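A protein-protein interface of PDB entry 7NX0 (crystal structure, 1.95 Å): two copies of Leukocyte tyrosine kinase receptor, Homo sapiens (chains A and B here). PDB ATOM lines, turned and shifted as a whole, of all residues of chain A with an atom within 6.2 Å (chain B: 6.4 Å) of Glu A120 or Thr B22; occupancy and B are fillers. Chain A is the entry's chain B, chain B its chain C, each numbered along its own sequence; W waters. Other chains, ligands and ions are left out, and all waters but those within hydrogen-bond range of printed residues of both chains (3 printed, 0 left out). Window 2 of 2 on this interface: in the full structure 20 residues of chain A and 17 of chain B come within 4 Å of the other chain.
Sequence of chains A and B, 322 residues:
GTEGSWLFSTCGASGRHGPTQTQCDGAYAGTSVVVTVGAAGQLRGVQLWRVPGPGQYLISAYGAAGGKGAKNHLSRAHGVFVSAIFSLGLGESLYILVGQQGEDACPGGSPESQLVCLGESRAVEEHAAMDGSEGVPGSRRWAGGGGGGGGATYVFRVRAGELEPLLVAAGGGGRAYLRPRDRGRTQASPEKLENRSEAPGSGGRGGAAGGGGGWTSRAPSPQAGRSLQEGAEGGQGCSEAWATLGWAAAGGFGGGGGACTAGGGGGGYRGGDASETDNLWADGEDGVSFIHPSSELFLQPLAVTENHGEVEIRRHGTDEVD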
ATOM      1  N   LYS A  71      -5.502  22.400 -13.377  1.00  0.00           N
ATOM      2  CA  LYS A  71      -4.827  23.426 -12.599  1.00  0.00           C
ATOM      3  C   LYS A  71      -5.662  23.787 -11.381  1.00  0.00           C
ATOM      4  O   LYS A  71      -5.680  24.936 -10.939  1.00  0.00           O
ATOM      5  CB  LYS A  71      -4.549  24.654 -13.463  1.00  0.00           C
ATOM      6  CG  LYS A  71      -3.554  24.361 -14.579  1.00  0.00           C
ATOM      7  CD  LYS A  71      -3.268  25.582 -15.430  1.00  0.00           C
ATOM      8  CE  LYS A  71      -2.434  25.208 -16.651  1.00  0.00           C
ATOM      9  NZ  LYS A  71      -2.032  26.402 -17.446  1.00  0.00           N
ATOM     10  N   LEU A 115       0.173  17.334 -21.752  1.00  0.00           N
ATOM     11  CA  LEU A 115       0.898  18.601 -21.746  1.00  0.00           C
ATOM     12  C   LEU A 115       0.200  19.634 -20.871  1.00  0.00           C
ATOM     13  O   LEU A 115       0.854  20.383 -20.136  1.00  0.00           O
ATOM     14  CB  LEU A 115       1.048  19.139 -23.172  1.00  0.00           C
ATOM     15  CG  LEU A 115       2.224  18.556 -23.950  1.00  0.00           C
ATOM     16  CD1 LEU A 115       2.296  19.087 -25.373  1.00  0.00           C
ATOM     17  CD2 LEU A 115       3.532  18.839 -23.199  1.00  0.00           C
ATOM     18  N   VAL A 116      -1.130  19.695 -20.939  1.00  0.00           N
ATOM     19  CA  VAL A 116      -1.871  20.651 -20.121  1.00  0.00           C
ATOM     20  C   VAL A 116      -1.674  20.336 -18.640  1.00  0.00           C
ATOM     21  O   VAL A 116      -1.547  21.238 -17.804  1.00  0.00           O
ATOM     22  CB  VAL A 116      -3.359  20.635 -20.520  1.00  0.00           C
ATOM     23  CG1 VAL A 116      -4.191  21.412 -19.523  1.00  0.00           C
ATOM     24  CG2 VAL A 116      -3.544  21.191 -21.947  1.00  0.00           C
ATOM     25  N   CYS A 117      -1.607  19.052 -18.305  1.00  0.00           N
ATOM     26  CA  CYS A 117      -1.450  18.635 -16.919  1.00  0.00           C
ATOM     27  C   CYS A 117      -0.085  19.006 -16.354  1.00  0.00           C
ATOM     28  O   CYS A 117       0.037  19.204 -15.142  1.00  0.00           O
ATOM     29  CB  CYS A 117      -1.668  17.131 -16.815  1.00  0.00           C
ATOM     30  SG  CYS A 117      -3.390  16.686 -17.045  1.00  0.00           S
ATOM     31  N   LEU A 118       0.943  19.082 -17.198  1.00  0.00           N
ATOM     32  CA  LEU A 118       2.269  19.469 -16.742  1.00  0.00           C
ATOM     33  C   LEU A 118       2.402  20.968 -16.541  1.00  0.00           C
ATOM     34  O   LEU A 118       3.424  21.424 -16.009  1.00  0.00           O
ATOM     35  CB  LEU A 118       3.319  18.997 -17.734  1.00  0.00           C
ATOM     36  CG  LEU A 118       3.587  17.494 -17.697  1.00  0.00           C
ATOM     37  CD1 LEU A 118       4.469  17.158 -18.886  1.00  0.00           C
ATOM     38  CD2 LEU A 118       4.219  17.080 -16.391  1.00  0.00           C
ATOM     39  N   GLY A 119       1.416  21.738 -16.997  1.00  0.00           N
ATOM     40  CA  GLY A 119       1.302  23.133 -16.663  1.00  0.00           C
ATOM     41  C   GLY A 119       1.958  24.093 -17.623  1.00  0.00           C
ATOM     42  O   GLY A 119       1.756  25.304 -17.483  1.00  0.00           O
ATOM     43  N   GLU A 120       2.737  23.609 -18.587  1.00  0.00           N
ATOM     44  CA  GLU A 120       3.435  24.529 -19.474  1.00  0.00           C
ATOM     45  C   GLU A 120       2.517  25.102 -20.551  1.00  0.00           C
ATOM     46  O   GLU A 120       2.804  26.184 -21.075  1.00  0.00           O
ATOM     47  CB  GLU A 120       4.636  23.844 -20.133  1.00  0.00           C
ATOM     48  CG  GLU A 120       5.722  23.369 -19.162  1.00  0.00           C
ATOM     49  CD  GLU A 120       6.322  24.488 -18.325  1.00  0.00           C
ATOM     50  OE1 GLU A 120       6.425  25.632 -18.819  1.00  0.00           O
ATOM     51  OE2 GLU A 120       6.699  24.218 -17.166  1.00  0.00           O
ATOM     52  N   SER A 121       1.422  24.410 -20.873  1.00  0.00           N
ATOM     53  CA  SER A 121       0.469  24.871 -21.879  1.00  0.00           C
ATOM     54  C   SER A 121      -0.560  25.796 -21.239  1.00  0.00           C
ATOM     55  O   SER A 121      -1.228  25.417 -20.270  1.00  0.00           O
ATOM     56  CB  SER A 121      -0.235  23.681 -22.539  1.00  0.00           C
ATOM     57  OG  SER A 121      -1.437  24.096 -23.175  1.00  0.00           O
ATOM     58  N   ARG A 122      -0.700  27.001 -21.794  1.00  0.00           N
ATOM     59  CA  ARG A 122      -1.753  27.933 -21.408  1.00  0.00           C
ATOM     60  C   ARG A 122      -2.751  28.180 -22.543  1.00  0.00           C
ATOM     61  O   ARG A 122      -3.442  29.205 -22.543  1.00  0.00           O
ATOM     62  CB  ARG A 122      -1.143  29.263 -20.953  1.00  0.00           C
ATOM     63  CG  ARG A 122      -0.181  29.182 -19.760  1.00  0.00           C
ATOM     64  CD  ARG A 122       0.269  30.594 -19.323  1.00  0.00           C
ATOM     65  NE  ARG A 122      -0.853  31.440 -18.909  1.00  0.00           N
ATOM     66  CZ  ARG A 122      -1.380  32.425 -19.640  1.00  0.00           C
ATOM     67  NH1 ARG A 122      -0.896  32.721 -20.843  1.00  0.00           N
ATOM     68  NH2 ARG A 122      -2.400  33.123 -19.162  1.00  0.00           N
ATOM     69  N   THR B  20       7.296  19.672 -11.246  1.00  0.00           N
ATOM     70  CA  THR B  20       8.149  20.757 -11.717  1.00  0.00           C
ATOM     71  C   THR B  20       7.855  22.044 -10.944  1.00  0.00           C
ATOM     72  O   THR B  20       6.837  22.169 -10.260  1.00  0.00           O
ATOM     73  CB  THR B  20       7.921  21.014 -13.207  1.00  0.00           C
ATOM     74  OG1 THR B  20       6.601  21.552 -13.350  1.00  0.00           O
ATOM     75  CG2 THR B  20       8.060  19.742 -14.006  1.00  0.00           C
ATOM     76  N   GLN B  21       8.738  23.040 -11.118  1.00  0.00           N
ATOM     77  CA  GLN B  21       8.513  24.358 -10.529  1.00  0.00           C
ATOM     78  C   GLN B  21       7.167  24.934 -10.964  1.00  0.00           C
ATOM     79  O   GLN B  21       6.417  25.485 -10.152  1.00  0.00           O
ATOM     80  CB  GLN B  21       9.640  25.315 -10.942  1.00  0.00           C
ATOM     81  CG  GLN B  21       9.613  26.653 -10.224  1.00  0.00           C
ATOM     82  CD  GLN B  21       9.965  26.481  -8.759  1.00  0.00           C
ATOM     83  OE1 GLN B  21      11.038  25.986  -8.429  1.00  0.00           O
ATOM     84  NE2 GLN B  21       9.039  26.841  -7.879  1.00  0.00           N
ATOM     85  N   THR B  22       6.858  24.843 -12.254  1.00  0.00           N
ATOM     86  CA  THR B  22       5.590  25.374 -12.736  1.00  0.00           C
ATOM     87  C   THR B  22       4.424  24.750 -11.992  1.00  0.00           C
ATOM     88  O   THR B  22       3.487  25.449 -11.589  1.00  0.00           O
ATOM     89  CB  THR B  22       5.459  25.136 -14.236  1.00  0.00           C
ATOM     90  OG1 THR B  22       6.481  25.886 -14.914  1.00  0.00           O
ATOM     91  CG2 THR B  22       4.091  25.574 -14.735  1.00  0.00           C
ATOM     92  N   GLN B  23       4.466  23.436 -11.792  1.00  0.00           N
ATOM     93  CA  GLN B  23       3.341  22.767 -11.154  1.00  0.00           C
ATOM     94  C   GLN B  23       3.187  23.228  -9.715  1.00  0.00           C
ATOM     95  O   GLN B  23       2.078  23.530  -9.267  1.00  0.00           O
ATOM     96  CB  GLN B  23       3.529  21.255 -11.225  1.00  0.00           C
ATOM     97  CG  GLN B  23       3.311  20.685 -12.612  1.00  0.00           C
ATOM     98  CD  GLN B  23       3.607  19.201 -12.683  1.00  0.00           C
ATOM     99  OE1 GLN B  23       4.732  18.763 -12.453  1.00  0.00           O
ATOM    100  NE2 GLN B  23       2.587  18.413 -13.030  1.00  0.00           N
ATOM    101  N   CYS B  24       4.287  23.320  -8.981  1.00  0.00           N
ATOM    102  CA  CYS B  24       4.169  23.736  -7.592  1.00  0.00           C
ATOM    103  C   CYS B  24       3.812  25.209  -7.479  1.00  0.00           C
ATOM    104  O   CYS B  24       3.021  25.584  -6.607  1.00  0.00           O
ATOM    105  CB  CYS B  24       5.452  23.413  -6.835  1.00  0.00           C
ATOM    106  SG  CYS B  24       5.689  21.638  -6.548  1.00  0.00           S
ATOM    107  N   ASP B  25       4.353  26.071  -8.355  1.00  0.00           N
ATOM    108  CA  ASP B  25       3.931  27.469  -8.312  1.00  0.00           C
ATOM    109  C   ASP B  25       2.424  27.576  -8.511  1.00  0.00           C
ATOM    110  O   ASP B  25       1.741  28.326  -7.804  1.00  0.00           O
ATOM    111  CB  ASP B  25       4.643  28.320  -9.377  1.00  0.00           C
ATOM    112  CG  ASP B  25       6.114  28.568  -9.047  1.00  0.00           C
ATOM    113  OD1 ASP B  25       6.550  28.214  -7.930  1.00  0.00           O
ATOM    114  OD2 ASP B  25       6.836  29.111  -9.911  1.00  0.00           O
ATOM    115  N   GLY B  26       1.880  26.817  -9.463  1.00  0.00           N
ATOM    116  CA  GLY B  26       0.443  26.821  -9.644  1.00  0.00           C
ATOM    117  C   GLY B  26      -0.296  26.302  -8.427  1.00  0.00           C
ATOM    118  O   GLY B  26      -1.331  26.848  -8.037  1.00  0.00           O
ATOM    119  N   ALA B  27       0.234  25.254  -7.800  1.00  0.00           N
ATOM    120  CA  ALA B  27      -0.451  24.644  -6.665  1.00  0.00           C
ATOM    121  C   ALA B  27      -0.521  25.588  -5.475  1.00  0.00           C
ATOM    122  O   ALA B  27      -1.560  25.690  -4.813  1.00  0.00           O
ATOM    123  CB  ALA B  27       0.255  23.347  -6.262  1.00  0.00           C
ATOM    124  N   VAL B  37      11.516  24.057  -6.534  1.00  0.00           N
ATOM    125  CA  VAL B  37      11.443  22.647  -6.907  1.00  0.00           C
ATOM    126  C   VAL B  37      12.747  22.285  -7.590  1.00  0.00           C
ATOM    127  O   VAL B  37      13.225  23.018  -8.462  1.00  0.00           O
ATOM    128  CB  VAL B  37      10.238  22.351  -7.818  1.00  0.00           C
ATOM    129  CG1 VAL B  37      10.235  20.851  -8.169  1.00  0.00           C
ATOM    130  CG2 VAL B  37       8.947  22.757  -7.133  1.00  0.00           C
HETATM  131  O   HOH W   1       5.917  21.746 -15.897  1.00  0.00           O
HETATM  132  O   HOH W   2       0.047  19.852 -11.819  1.00  0.00           O
HETATM  133  O   HOH W   3      -4.078  25.554  -8.649  1.00  0.00           O
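Leu A118 touches Gln B23. Gly A119 touches Thr B22.
No position is printed for both chains. Of the 4 pairs that touch across the chains among the printed residues, none has its exchanged pair printed and touching as well.
Printed residues of chain B within 4 Å of Cys A117: Gln B23 (3.4 Å). Of the printed residues of chain B, Leu A118 touches Gln B23. Of the printed residues of chain B, Gly A119 touches Thr B22. Thr B20 touches none of the printed residues of chain A. Of chain A, only Gly A119 (3.6 Å) and Glu A120 (2.8 Å) come within 4 Å of Thr B22. Ala B27 touches none of the printed residues of chain A. The nearest residue of chain B that does not touch Glu A120 is Thr B20 (4.7 Å). The nearest residue of chain A that does not touch Thr B22 is Leu A118 (4.4 Å).
Of the 9 printed residues of chain A, 4 touch a printed residue of chain B. Printed residues of chain A that touch a printed residue of chain B: Cys A117, Leu A118, Gly A119 and Glu A120. Hydrophobic or aromatic side chains of chain A within 4 Å of the printed part of chain B: Leu A118. Among the printed residues, 4 pairs touch across the chains. Among the printed residues, no Asp or Glu carboxylate lies within 4 Å of a Lys or Arg side-chain nitrogen of the other chain.
The backbone NH (N) of Thr B22 lies close to the side-chain hydroxyl (OG1) of Thr B20 (3.5 Å). The backbone NH (N) of Thr B20 lies within hydrogen-bond range of the side-chain amide oxygen (OE1) of Gln B23.
Water W1 lies within hydrogen-bond range of the backbone carbonyl oxygen (O) of Leu A118 (2.5 Å), the side-chain hydroxyl (OG1) of Thr B20 (2.6 Å) and the side-chain carboxylate (OE2) of Glu A120 (2.9 Å). Water W3 bridges O of Lys A71 (2.9 Å) and O of Gly B26 (3.1 Å). Water W2 bridges the side-chain amide nitrogen (NE2) of Gln B23 and the backbone carbonyl oxygen (O) of Cys A117.
The side-chain amide nitrogen (NE2) of Gln B23 sits at hydrogen-bond distance from the backbone carbonyl oxygen (O) of Cys A117, 3.4 Å away. The side-chain carboxylate (OE2) of Glu A120 lies within hydrogen-bond range of the side-chain hydroxyl (OG1) of Thr B22.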
